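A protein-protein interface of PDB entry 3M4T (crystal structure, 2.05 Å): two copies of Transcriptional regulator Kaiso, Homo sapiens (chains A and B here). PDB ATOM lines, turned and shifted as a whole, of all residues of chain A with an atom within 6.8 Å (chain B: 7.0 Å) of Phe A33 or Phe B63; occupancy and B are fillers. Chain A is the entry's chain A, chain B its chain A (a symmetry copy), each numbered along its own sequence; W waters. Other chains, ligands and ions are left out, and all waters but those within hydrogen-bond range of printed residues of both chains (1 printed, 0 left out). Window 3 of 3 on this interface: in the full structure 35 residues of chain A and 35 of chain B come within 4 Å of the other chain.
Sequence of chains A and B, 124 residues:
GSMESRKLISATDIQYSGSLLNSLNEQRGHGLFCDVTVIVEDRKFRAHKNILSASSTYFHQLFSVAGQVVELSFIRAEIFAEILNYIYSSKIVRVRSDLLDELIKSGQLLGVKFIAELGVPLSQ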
ATOM      1  N   GLN A  27     -22.686  -3.698   3.681  1.00  0.00           N
ATOM      2  CA  GLN A  27     -22.757  -4.377   4.993  1.00  0.00           C
ATOM      3  C   GLN A  27     -23.683  -3.639   5.953  1.00  0.00           C
ATOM      4  O   GLN A  27     -24.501  -4.254   6.683  1.00  0.00           O
ATOM      5  CB  GLN A  27     -21.352  -4.423   5.606  1.00  0.00           C
ATOM      6  CG  GLN A  27     -20.346  -5.384   4.914  1.00  0.00           C
ATOM      7  CD  GLN A  27     -18.952  -5.166   5.490  1.00  0.00           C
ATOM      8  OE1 GLN A  27     -18.845  -4.567   6.539  1.00  0.00           O
ATOM      9  NE2 GLN A  27     -17.902  -5.647   4.822  1.00  0.00           N
ATOM     10  N   HIS A  30     -27.359  -4.201   5.609  1.00  0.00           N
ATOM     11  CA  HIS A  30     -27.778  -5.550   6.085  1.00  0.00           C
ATOM     12  C   HIS A  30     -27.618  -5.671   7.589  1.00  0.00           C
ATOM     13  O   HIS A  30     -28.057  -6.649   8.172  1.00  0.00           O
ATOM     14  CB  HIS A  30     -26.901  -6.668   5.483  1.00  0.00           C
ATOM     15  CG  HIS A  30     -27.157  -6.940   4.039  1.00  0.00           C
ATOM     16  ND1 HIS A  30     -28.358  -7.442   3.574  1.00  0.00           N
ATOM     17  CD2 HIS A  30     -26.372  -6.765   2.949  1.00  0.00           C
ATOM     18  CE1 HIS A  30     -28.302  -7.561   2.258  1.00  0.00           C
ATOM     19  NE2 HIS A  30     -27.113  -7.144   1.851  1.00  0.00           N
ATOM     20  N   GLY A  31     -26.922  -4.705   8.192  1.00  0.00           N
ATOM     21  CA  GLY A  31     -26.501  -4.783   9.588  1.00  0.00           C
ATOM     22  C   GLY A  31     -25.335  -5.717   9.794  1.00  0.00           C
ATOM     23  O   GLY A  31     -25.050  -6.133  10.920  1.00  0.00           O
ATOM     24  N   LEU A  32     -24.624  -6.050   8.716  1.00  0.00           N
ATOM     25  CA  LEU A  32     -23.580  -7.065   8.818  1.00  0.00           C
ATOM     26  C   LEU A  32     -22.351  -6.536   9.543  1.00  0.00           C
ATOM     27  O   LEU A  32     -21.817  -5.487   9.176  1.00  0.00           O
ATOM     28  CB  LEU A  32     -23.213  -7.537   7.412  1.00  0.00           C
ATOM     29  CG  LEU A  32     -22.373  -8.792   7.239  1.00  0.00           C
ATOM     30  CD1 LEU A  32     -23.030 -10.003   7.865  1.00  0.00           C
ATOM     31  CD2 LEU A  32     -22.164  -8.990   5.722  1.00  0.00           C
ATOM     32  N   PHE A  33     -21.904  -7.257  10.573  1.00  0.00           N
ATOM     33  CA  PHE A  33     -20.745  -6.876  11.428  1.00  0.00           C
ATOM     34  C   PHE A  33     -21.013  -5.611  12.270  1.00  0.00           C
ATOM     35  O   PHE A  33     -20.114  -5.110  12.952  1.00  0.00           O
ATOM     36  CB  PHE A  33     -19.431  -6.714  10.618  1.00  0.00           C
ATOM     37  CG  PHE A  33     -19.127  -7.891   9.730  1.00  0.00           C
ATOM     38  CD1 PHE A  33     -18.901  -9.159  10.286  1.00  0.00           C
ATOM     39  CD2 PHE A  33     -19.100  -7.747   8.351  1.00  0.00           C
ATOM     40  CE1 PHE A  33     -18.660 -10.234   9.468  1.00  0.00           C
ATOM     41  CE2 PHE A  33     -18.842  -8.818   7.535  1.00  0.00           C
ATOM     42  CZ  PHE A  33     -18.622 -10.077   8.091  1.00  0.00           C
ATOM     43  N   CYS A  34     -22.244  -5.109  12.225  1.00  0.00           N
ATOM     44  CA  CYS A  34     -22.567  -3.876  12.947  1.00  0.00           C
ATOM     45  C   CYS A  34     -22.578  -4.217  14.422  1.00  0.00           C
ATOM     46  O   CYS A  34     -23.203  -5.175  14.825  1.00  0.00           O
ATOM     47  CB  CYS A  34     -23.873  -3.273  12.469  1.00  0.00           C
ATOM     48  SG  CYS A  34     -23.792  -2.567  10.825  1.00  0.00           S
ATOM     49  N   ASP A  35     -21.809  -3.468  15.198  1.00  0.00           N
ATOM     50  CA  ASP A  35     -21.575  -3.756  16.613  1.00  0.00           C
ATOM     51  C   ASP A  35     -22.070  -2.614  17.519  1.00  0.00           C
ATOM     52  O   ASP A  35     -21.740  -2.566  18.707  1.00  0.00           O
ATOM     53  CB  ASP A  35     -20.088  -4.014  16.858  1.00  0.00           C
ATOM     54  CG  ASP A  35     -19.190  -2.915  16.285  1.00  0.00           C
ATOM     55  OD1 ASP A  35     -19.712  -1.971  15.639  1.00  0.00           O
ATOM     56  OD2 ASP A  35     -17.957  -3.005  16.488  1.00  0.00           O
ATOM     57  N   VAL A  36     -22.856  -1.704  16.939  1.00  0.00           N
ATOM     58  CA  VAL A  36     -23.458  -0.600  17.681  1.00  0.00           C
ATOM     59  C   VAL A  36     -24.751  -0.250  16.987  1.00  0.00           C
ATOM     60  O   VAL A  36     -24.832  -0.295  15.755  1.00  0.00           O
ATOM     61  CB  VAL A  36     -22.517   0.646  17.789  1.00  0.00           C
ATOM     62  CG1 VAL A  36     -22.321   1.343  16.419  1.00  0.00           C
ATOM     63  CG2 VAL A  36     -23.032   1.692  18.843  1.00  0.00           C
ATOM     64  N   ARG A  46     -28.015   0.925  12.591  1.00  0.00           N
ATOM     65  CA  ARG A  46     -26.956  -0.066  12.842  1.00  0.00           C
ATOM     66  C   ARG A  46     -25.733   0.456  12.114  1.00  0.00           C
ATOM     67  O   ARG A  46     -25.858   0.960  10.996  1.00  0.00           O
ATOM     68  CB  ARG A  46     -27.357  -1.463  12.334  1.00  0.00           C
ATOM     69  CG  ARG A  46     -28.585  -2.055  13.073  1.00  0.00           C
ATOM     70  CD  ARG A  46     -28.788  -3.594  12.806  1.00  0.00           C
ATOM     71  NE  ARG A  46     -27.606  -4.391  13.190  1.00  0.00           N
ATOM     72  CZ  ARG A  46     -27.494  -5.725  13.076  1.00  0.00           C
ATOM     73  NH1 ARG A  46     -28.503  -6.474  12.601  1.00  0.00           N
ATOM     74  NH2 ARG A  46     -26.369  -6.317  13.456  1.00  0.00           N
ATOM     75  N   ALA A  47     -24.562   0.359  12.750  1.00  0.00           N
ATOM     76  CA  ALA A  47     -23.312   0.848  12.137  1.00  0.00           C
ATOM     77  C   ALA A  47     -22.138   0.110  12.777  1.00  0.00           C
ATOM     78  O   ALA A  47     -22.330  -0.734  13.696  1.00  0.00           O
ATOM     79  CB  ALA A  47     -23.188   2.391  12.354  1.00  0.00           C
ATOM     80  N   HIS A  48     -20.928   0.408  12.302  1.00  0.00           N
ATOM     81  CA  HIS A  48     -19.728  -0.231  12.779  1.00  0.00           C
ATOM     82  C   HIS A  48     -18.970   0.805  13.608  1.00  0.00           C
ATOM     83  O   HIS A  48     -18.647   1.889  13.109  1.00  0.00           O
ATOM     84  CB  HIS A  48     -18.814  -0.657  11.611  1.00  0.00           C
ATOM     85  CG  HIS A  48     -19.525  -1.341  10.487  1.00  0.00           C
ATOM     86  ND1 HIS A  48     -19.739  -2.710  10.456  1.00  0.00           N
ATOM     87  CD2 HIS A  48     -20.068  -0.850   9.349  1.00  0.00           C
ATOM     88  CE1 HIS A  48     -20.366  -3.031   9.335  1.00  0.00           C
ATOM     89  NE2 HIS A  48     -20.575  -1.922   8.642  1.00  0.00           N
ATOM     90  N   LYS A  49     -18.659   0.448  14.849  1.00  0.00           N
ATOM     91  CA  LYS A  49     -17.871   1.297  15.738  1.00  0.00           C
ATOM     92  C   LYS A  49     -16.539   1.733  15.176  1.00  0.00           C
ATOM     93  O   LYS A  49     -16.114   2.870  15.420  1.00  0.00           O
ATOM     94  CB  LYS A  49     -17.623   0.570  17.074  1.00  0.00           C
ATOM     95  CG  LYS A  49     -18.816   0.528  18.009  1.00  0.00           C
ATOM     96  CD  LYS A  49     -18.395  -0.185  19.319  1.00  0.00           C
ATOM     97  CE  LYS A  49     -19.542  -0.226  20.298  1.00  0.00           C
ATOM     98  NZ  LYS A  49     -19.053  -0.934  21.521  1.00  0.00           N
ATOM     99  N   ASN A  50     -15.820   0.851  14.457  1.00  0.00           N
ATOM    100  CA  ASN A  50     -14.501   1.243  13.943  1.00  0.00           C
ATOM    101  C   ASN A  50     -14.585   2.398  12.954  1.00  0.00           C
ATOM    102  O   ASN A  50     -13.769   3.330  13.023  1.00  0.00           O
ATOM    103  CB  ASN A  50     -13.649   0.054  13.363  1.00  0.00           C
ATOM    104  CG  ASN A  50     -14.305  -0.655  12.150  1.00  0.00           C
ATOM    105  OD1 ASN A  50     -15.485  -0.509  11.887  1.00  0.00           O
ATOM    106  ND2 ASN A  50     -13.515  -1.465  11.432  1.00  0.00           N
ATOM    107  N   ASP B  35     -12.384  -7.691  16.055  1.00  0.00           N
ATOM    108  CA  ASP B  35     -13.367  -8.714  16.410  1.00  0.00           C
ATOM    109  C   ASP B  35     -13.003 -10.088  15.816  1.00  0.00           C
ATOM    110  O   ASP B  35     -13.829 -11.004  15.800  1.00  0.00           O
ATOM    111  CB  ASP B  35     -14.760  -8.291  15.943  1.00  0.00           C
ATOM    112  CG  ASP B  35     -14.792  -7.874  14.470  1.00  0.00           C
ATOM    113  OD1 ASP B  35     -13.719  -7.853  13.814  1.00  0.00           O
ATOM    114  OD2 ASP B  35     -15.902  -7.568  13.976  1.00  0.00           O
ATOM    115  N   VAL B  36     -11.766 -10.207  15.329  1.00  0.00           N
ATOM    116  CA  VAL B  36     -11.251 -11.463  14.793  1.00  0.00           C
ATOM    117  C   VAL B  36      -9.760 -11.465  15.017  1.00  0.00           C
ATOM    118  O   VAL B  36      -9.108 -10.421  14.901  1.00  0.00           O
ATOM    119  CB  VAL B  36     -11.599 -11.669  13.281  1.00  0.00           C
ATOM    120  CG1 VAL B  36     -10.831 -10.676  12.372  1.00  0.00           C
ATOM    121  CG2 VAL B  36     -11.326 -13.140  12.802  1.00  0.00           C
ATOM    122  N   THR B  37      -9.228 -12.632  15.379  1.00  0.00           N
ATOM    123  CA  THR B  37      -7.808 -12.893  15.333  1.00  0.00           C
ATOM    124  C   THR B  37      -7.548 -13.882  14.179  1.00  0.00           C
ATOM    125  O   THR B  37      -8.241 -14.908  14.066  1.00  0.00           O
ATOM    126  CB  THR B  37      -7.331 -13.486  16.679  1.00  0.00           C
ATOM    127  OG1 THR B  37      -7.707 -12.600  17.739  1.00  0.00           O
ATOM    128  CG2 THR B  37      -5.831 -13.696  16.698  1.00  0.00           C
ATOM    129  N   VAL B  38      -6.591 -13.534  13.308  1.00  0.00           N
ATOM    130  CA  VAL B  38      -6.169 -14.415  12.206  1.00  0.00           C
ATOM    131  C   VAL B  38      -4.818 -14.980  12.583  1.00  0.00           C
ATOM    132  O   VAL B  38      -3.844 -14.222  12.752  1.00  0.00           O
ATOM    133  CB  VAL B  38      -6.037 -13.647  10.826  1.00  0.00           C
ATOM    134  CG1 VAL B  38      -5.690 -14.640   9.684  1.00  0.00           C
ATOM    135  CG2 VAL B  38      -7.336 -12.915  10.484  1.00  0.00           C
ATOM    136  N   HIS B  48     -10.258  -6.299  11.844  1.00  0.00           N
ATOM    137  CA  HIS B  48     -11.675  -6.040  11.880  1.00  0.00           C
ATOM    138  C   HIS B  48     -12.306  -6.854  10.751  1.00  0.00           C
ATOM    139  O   HIS B  48     -11.925  -6.704   9.584  1.00  0.00           O
ATOM    140  CB  HIS B  48     -11.983  -4.552  11.614  1.00  0.00           C
ATOM    141  CG  HIS B  48     -11.117  -3.596  12.372  1.00  0.00           C
ATOM    142  ND1 HIS B  48     -11.429  -3.149  13.646  1.00  0.00           N
ATOM    143  CD2 HIS B  48      -9.951  -2.997  12.038  1.00  0.00           C
ATOM    144  CE1 HIS B  48     -10.499  -2.298  14.052  1.00  0.00           C
ATOM    145  NE2 HIS B  48      -9.592  -2.183  13.094  1.00  0.00           N
ATOM    146  N   LYS B  49     -13.290  -7.676  11.100  1.00  0.00           N
ATOM    147  CA  LYS B  49     -14.042  -8.461  10.125  1.00  0.00           C
ATOM    148  C   LYS B  49     -14.665  -7.655   9.011  1.00  0.00           C
ATOM    149  O   LYS B  49     -14.709  -8.124   7.867  1.00  0.00           O
ATOM    150  CB  LYS B  49     -15.157  -9.252  10.837  1.00  0.00           C
ATOM    151  CG  LYS B  49     -14.683 -10.471  11.605  1.00  0.00           C
ATOM    152  CD  LYS B  49     -15.917 -11.182  12.217  1.00  0.00           C
ATOM    153  CE  LYS B  49     -15.501 -12.424  12.967  1.00  0.00           C
ATOM    154  NZ  LYS B  49     -16.745 -13.038  13.527  1.00  0.00           N
ATOM    155  N   ASN B  50     -15.203  -6.456   9.303  1.00  0.00           N
ATOM    156  CA  ASN B  50     -15.855  -5.680   8.240  1.00  0.00           C
ATOM    157  C   ASN B  50     -14.885  -5.283   7.134  1.00  0.00           C
ATOM    158  O   ASN B  50     -15.228  -5.385   5.946  1.00  0.00           O
ATOM    159  CB  ASN B  50     -16.678  -4.440   8.752  1.00  0.00           C
ATOM    160  CG  ASN B  50     -15.821  -3.380   9.490  1.00  0.00           C
ATOM    161  OD1 ASN B  50     -14.703  -3.635   9.901  1.00  0.00           O
ATOM    162  ND2 ASN B  50     -16.390  -2.181   9.685  1.00  0.00           N
ATOM    163  N   ILE B  51     -13.697  -4.810   7.518  1.00  0.00           N
ATOM    164  CA  ILE B  51     -12.679  -4.414   6.549  1.00  0.00           C
ATOM    165  C   ILE B  51     -12.186  -5.661   5.764  1.00  0.00           C
ATOM    166  O   ILE B  51     -12.021  -5.603   4.532  1.00  0.00           O
ATOM    167  CB  ILE B  51     -11.435  -3.720   7.229  1.00  0.00           C
ATOM    168  CG1 ILE B  51     -11.801  -2.483   8.116  1.00  0.00           C
ATOM    169  CG2 ILE B  51     -10.398  -3.267   6.196  1.00  0.00           C
ATOM    170  CD1 ILE B  51     -12.693  -1.468   7.428  1.00  0.00           C
ATOM    171  N   LEU B  52     -11.895  -6.757   6.481  1.00  0.00           N
ATOM    172  CA  LEU B  52     -11.415  -7.989   5.815  1.00  0.00           C
ATOM    173  C   LEU B  52     -12.473  -8.526   4.856  1.00  0.00           C
ATOM    174  O   LEU B  52     -12.171  -8.842   3.711  1.00  0.00           O
ATOM    175  CB  LEU B  52     -11.018  -9.079   6.832  1.00  0.00           C
ATOM    176  CG  LEU B  52      -9.861  -8.851   7.793  1.00  0.00           C
ATOM    177  CD1 LEU B  52      -9.325 -10.096   8.532  1.00  0.00           C
ATOM    178  CD2 LEU B  52      -8.754  -8.034   7.216  1.00  0.00           C
ATOM    179  N   SER B  53     -13.725  -8.569   5.288  1.00  0.00           N
ATOM    180  CA  SER B  53     -14.796  -9.053   4.406  1.00  0.00           C
ATOM    181  C   SER B  53     -14.994  -8.193   3.133  1.00  0.00           C
ATOM    182  O   SER B  53     -15.259  -8.720   2.032  1.00  0.00           O
ATOM    183  CB  SER B  53     -16.111  -9.182   5.196  1.00  0.00           C
ATOM    184  OG  SER B  53     -17.196  -9.342   4.290  1.00  0.00           O
ATOM    185  N   ALA B  54     -14.896  -6.872   3.287  1.00  0.00           N
ATOM    186  CA  ALA B  54     -15.023  -5.941   2.163  1.00  0.00           C
ATOM    187  C   ALA B  54     -13.858  -6.013   1.161  1.00  0.00           C
ATOM    188  O   ALA B  54     -14.018  -5.675   0.006  1.00  0.00           O
ATOM    189  CB  ALA B  54     -15.140  -4.491   2.719  1.00  0.00           C
ATOM    190  N   TYR B  58     -12.232 -14.232  -0.136  1.00  0.00           N
ATOM    191  CA  TYR B  58     -12.129 -15.326   0.834  1.00  0.00           C
ATOM    192  C   TYR B  58     -12.690 -14.979   2.235  1.00  0.00           C
ATOM    193  O   TYR B  58     -13.493 -15.719   2.805  1.00  0.00           O
ATOM    194  CB  TYR B  58     -10.687 -15.794   0.968  1.00  0.00           C
ATOM    195  CG  TYR B  58     -10.594 -16.950   1.908  1.00  0.00           C
ATOM    196  CD1 TYR B  58     -11.012 -18.236   1.521  1.00  0.00           C
ATOM    197  CD2 TYR B  58     -10.125 -16.772   3.195  1.00  0.00           C
ATOM    198  CE1 TYR B  58     -10.947 -19.305   2.427  1.00  0.00           C
ATOM    199  CE2 TYR B  58     -10.063 -17.835   4.086  1.00  0.00           C
ATOM    200  CZ  TYR B  58     -10.482 -19.076   3.698  1.00  0.00           C
ATOM    201  OH  TYR B  58     -10.396 -20.080   4.636  1.00  0.00           O
ATOM    202  N   PHE B  59     -12.241 -13.869   2.818  1.00  0.00           N
ATOM    203  CA  PHE B  59     -12.774 -13.432   4.108  1.00  0.00           C
ATOM    204  C   PHE B  59     -14.268 -13.122   4.043  1.00  0.00           C
ATOM    205  O   PHE B  59     -14.974 -13.339   5.018  1.00  0.00           O
ATOM    206  CB  PHE B  59     -12.014 -12.219   4.610  1.00  0.00           C
ATOM    207  CG  PHE B  59     -10.665 -12.548   5.185  1.00  0.00           C
ATOM    208  CD1 PHE B  59     -10.538 -13.581   6.137  1.00  0.00           C
ATOM    209  CD2 PHE B  59      -9.549 -11.829   4.819  1.00  0.00           C
ATOM    210  CE1 PHE B  59      -9.290 -13.889   6.691  1.00  0.00           C
ATOM    211  CE2 PHE B  59      -8.299 -12.113   5.371  1.00  0.00           C
ATOM    212  CZ  PHE B  59      -8.177 -13.164   6.311  1.00  0.00           C
ATOM    213  N   HIS B  60     -14.737 -12.598   2.906  1.00  0.00           N
ATOM    214  CA  HIS B  60     -16.169 -12.354   2.714  1.00  0.00           C
ATOM    215  C   HIS B  60     -16.959 -13.668   2.897  1.00  0.00           C
ATOM    216  O   HIS B  60     -17.962 -13.709   3.627  1.00  0.00           O
ATOM    217  CB  HIS B  60     -16.434 -11.732   1.330  1.00  0.00           C
ATOM    218  CG  HIS B  60     -17.883 -11.447   1.058  1.00  0.00           C
ATOM    219  ND1 HIS B  60     -18.645 -10.610   1.844  1.00  0.00           N
ATOM    220  CD2 HIS B  60     -18.709 -11.885   0.078  1.00  0.00           C
ATOM    221  CE1 HIS B  60     -19.878 -10.560   1.376  1.00  0.00           C
ATOM    222  NE2 HIS B  60     -19.940 -11.310   0.294  1.00  0.00           N
ATOM    223  N   GLN B  61     -16.499 -14.737   2.252  1.00  0.00           N
ATOM    224  CA  GLN B  61     -17.140 -16.047   2.425  1.00  0.00           C
ATOM    225  C   GLN B  61     -16.947 -16.549   3.854  1.00  0.00           C
ATOM    226  O   GLN B  61     -17.919 -16.943   4.533  1.00  0.00           O
ATOM    227  CB  GLN B  61     -16.616 -17.062   1.391  1.00  0.00           C
ATOM    228  CG  GLN B  61     -17.286 -18.489   1.505  1.00  0.00           C
ATOM    229  CD  GLN B  61     -18.840 -18.452   1.479  1.00  0.00           C
ATOM    230  OE1 GLN B  61     -19.458 -17.629   0.771  1.00  0.00           O
ATOM    231  NE2 GLN B  61     -19.470 -19.352   2.261  1.00  0.00           N
ATOM    232  N   LEU B  62     -15.705 -16.512   4.331  1.00  0.00           N
ATOM    233  CA  LEU B  62     -15.387 -17.074   5.632  1.00  0.00           C
ATOM    234  C   LEU B  62     -16.187 -16.448   6.776  1.00  0.00           C
ATOM    235  O   LEU B  62     -16.717 -17.181   7.622  1.00  0.00           O
ATOM    236  CB  LEU B  62     -13.883 -17.004   5.890  1.00  0.00           C
ATOM    237  CG  LEU B  62     -13.319 -17.506   7.208  1.00  0.00           C
ATOM    238  CD1 LEU B  62     -13.481 -19.026   7.314  1.00  0.00           C
ATOM    239  CD2 LEU B  62     -11.860 -17.110   7.290  1.00  0.00           C
ATOM    240  N   PHE B  63     -16.343 -15.118   6.774  1.00  0.00           N
ATOM    241  CA  PHE B  63     -17.022 -14.452   7.897  1.00  0.00           C
ATOM    242  C   PHE B  63     -18.556 -14.462   7.857  1.00  0.00           C
ATOM    243  O   PHE B  63     -19.219 -13.867   8.724  1.00  0.00           O
ATOM    244  CB  PHE B  63     -16.480 -13.032   8.107  1.00  0.00           C
ATOM    245  CG  PHE B  63     -15.025 -12.991   8.513  1.00  0.00           C
ATOM    246  CD1 PHE B  63     -14.500 -13.936   9.389  1.00  0.00           C
ATOM    247  CD2 PHE B  63     -14.175 -12.016   8.012  1.00  0.00           C
ATOM    248  CE1 PHE B  63     -13.151 -13.904   9.765  1.00  0.00           C
ATOM    249  CE2 PHE B  63     -12.828 -11.977   8.390  1.00  0.00           C
ATOM    250  CZ  PHE B  63     -12.322 -12.929   9.267  1.00  0.00           C
ATOM    251  N   SER B  64     -19.131 -15.146   6.868  1.00  0.00           N
ATOM    252  CA  SER B  64     -20.570 -15.393   6.886  1.00  0.00           C
ATOM    253  C   SER B  64     -20.897 -16.432   7.956  1.00  0.00           C
ATOM    254  O   SER B  64     -22.052 -16.591   8.328  1.00  0.00           O
ATOM    255  CB  SER B  64     -21.095 -15.831   5.517  1.00  0.00           C
ATOM    256  OG  SER B  64     -20.615 -17.132   5.196  1.00  0.00           O
ATOM    257  N   VAL B  65     -19.889 -17.118   8.484  1.00  0.00           N
ATOM    258  CA  VAL B  65     -20.152 -18.100   9.525  1.00  0.00           C
ATOM    259  C   VAL B  65     -19.349 -17.815  10.785  1.00  0.00           C
ATOM    260  O   VAL B  65     -19.921 -17.734  11.886  1.00  0.00           O
ATOM    261  CB  VAL B  65     -19.912 -19.569   9.044  1.00  0.00           C
ATOM    262  CG1 VAL B  65     -20.483 -19.792   7.644  1.00  0.00           C
ATOM    263  CG2 VAL B  65     -18.450 -19.930   9.058  1.00  0.00           C
ATOM    264  N   ALA B  66     -18.049 -17.570  10.584  1.00  0.00           N
ATOM    265  CA  ALA B  66     -16.969 -17.810  11.574  1.00  0.00           C
ATOM    266  C   ALA B  66     -17.184 -17.338  13.021  1.00  0.00           C
ATOM    267  O   ALA B  66     -18.156 -16.642  13.334  1.00  0.00           O
ATOM    268  CB  ALA B  66     -15.623 -17.292  11.021  1.00  0.00           C
ATOM    269  N   GLY B  67     -16.270 -17.753  13.897  1.00  0.00           N
ATOM    270  CA  GLY B  67     -16.233 -17.281  15.266  1.00  0.00           C
ATOM    271  C   GLY B  67     -15.257 -16.129  15.347  1.00  0.00           C
ATOM    272  O   GLY B  67     -15.211 -15.273  14.466  1.00  0.00           O
ATOM    273  N   GLN B  68     -14.449 -16.133  16.394  1.00  0.00           N
ATOM    274  CA  GLN B  68     -13.570 -15.011  16.684  1.00  0.00           C
ATOM    275  C   GLN B  68     -12.126 -15.297  16.319  1.00  0.00           C
ATOM    276  O   GLN B  68     -11.286 -14.395  16.358  1.00  0.00           O
ATOM    277  CB  GLN B  68     -13.692 -14.634  18.155  1.00  0.00           C
ATOM    278  CG  GLN B  68     -15.147 -14.546  18.642  1.00  0.00           C
ATOM    279  CD  GLN B  68     -15.247 -14.161  20.099  1.00  0.00           C
ATOM    280  OE1 GLN B  68     -14.578 -14.745  20.973  1.00  0.00           O
ATOM    281  NE2 GLN B  68     -16.093 -13.170  20.380  1.00  0.00           N
ATOM    282  N   VAL B  69     -11.824 -16.559  15.996  1.00  0.00           N
ATOM    283  CA  VAL B  69     -10.462 -16.962  15.631  1.00  0.00           C
ATOM    284  C   VAL B  69     -10.493 -17.811  14.355  1.00  0.00           C
ATOM    285  O   VAL B  69     -11.253 -18.785  14.250  1.00  0.00           O
ATOM    286  CB  VAL B  69      -9.752 -17.746  16.762  1.00  0.00           C
ATOM    287  CG1 VAL B  69      -8.327 -18.022  16.370  1.00  0.00           C
ATOM    288  CG2 VAL B  69      -9.776 -16.972  18.097  1.00  0.00           C
ATOM    289  N   VAL B  70      -9.691 -17.426  13.372  1.00  0.00           N
ATOM    290  CA  VAL B  70      -9.634 -18.159  12.114  1.00  0.00           C
ATOM    291  C   VAL B  70      -8.180 -18.414  11.805  1.00  0.00           C
ATOM    292  O   VAL B  70      -7.271 -17.705  12.300  1.00  0.00           O
ATOM    293  CB  VAL B  70     -10.338 -17.419  10.923  1.00  0.00           C
ATOM    294  CG1 VAL B  70     -11.867 -17.377  11.128  1.00  0.00           C
ATOM    295  CG2 VAL B  70      -9.777 -16.023  10.703  1.00  0.00           C
HETATM  296  O   HOH W   1     -18.435  -7.508   2.594  1.00  0.00           O
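Among the printed residues, pairs that only touch across the chains: Gln A27 with Ala B54 (3.6 Å), Phe A33 with Ser B53 (3.6 Å), Phe A33 with Phe B63 (3.6 Å), Phe A33 with Lys B49 (3.8 Å), Gln A27 with Ser B53 (3.8 Å), Phe A33 with Asn B50 (3.8 Å) and Asn A50 with Ile B51 (3.9 Å).
The backbone carbonyl oxygen (O) of Gln A27 lies within hydrogen-bond range of the backbone NH (N) of Leu A32 (2.7 Å).
The backbone carbonyl oxygen (O) of Phe A33 lies within hydrogen-bond range of a ring nitrogen (ND1) of His A48, at 3.5 Å.
The side-chain hydroxyl (OG) of Ser B53 lies within hydrogen-bond range of a ring nitrogen (ND1) of His B60 (3.1 Å).
O of Gly B67 sits at hydrogen-bond distance from NZ of Lys B49 (2.9 Å).
The backbone NH of Lys B49 lies within hydrogen-bond range of the side-chain carboxylate of Asp B35 (2.8 Å).
His A48 touches Asn B50, and with the chains exchanged Asn A50 touches His B48.
Asn A50 touches its own counterpart, Asn B50.
Water W1 lies within hydrogen-bond range of the side-chain hydroxyl of Ser B53, the side-chain amide nitrogen of Gln A27 and a ring nitrogen (ND1) of His B60.
NE2 of Gln A27 sits at hydrogen-bond distance from O of Asn B50 (2.9 Å).
A ring nitrogen (ND1) of His B48 lies close to the side-chain amide nitrogen (ND2) of Asn A50, at 3.5 Å.
The side-chain amide oxygen (OD1) of Asn A50 sits at hydrogen-bond distance from the side-chain amide nitrogen (ND2) of Asn B50.
ND2 of Asn B50 lies close to ND1 of His A48, 3.5 Å away.
Of the printed residues of chain B, Gln A27 touches Asn B50, Ser B53 and Ala B54.
Phe A33 touches four residues of chain B.
Of the printed residues of chain B, His A48 touches Asn B50 (3.3 Å).
Of the printed residues of chain A, Ile B51 touches Asn A50 (3.9 Å).
Of the printed residues of chain A, Ser B53 touches Gln A27 (3.8 Å) and Phe A33 (3.6 Å).
Of chain A, only Phe A33 comes within 4 Å of Phe B63.
The nearest residue of chain B that does not touch Phe A33 is Asp B35 (4.9 Å).
The nearest residue of chain A that does not touch Phe B63 is Leu A32 (5.5 Å).
Of the 24 printed residues of chain B, 7 touch a printed residue of chain A.
Printed residues of chain B that touch a printed residue of chain A: His B48, Lys B49, Asn B50, Ile B51, Ser B53, Ala B54 and Phe B63.
Hydrophobic or aromatic side chains of chain B that line the printed part of chain A: His B48, Ile B51, Ala B54 and Phe B63.
Hydrophobic or aromatic side chains of chain A that line the printed part of chain B: Phe A33 and His A48.
Among the printed residues, no Asp or Glu carboxylate lies within 4 Å of a Lys or Arg side-chain nitrogen of the other chain.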
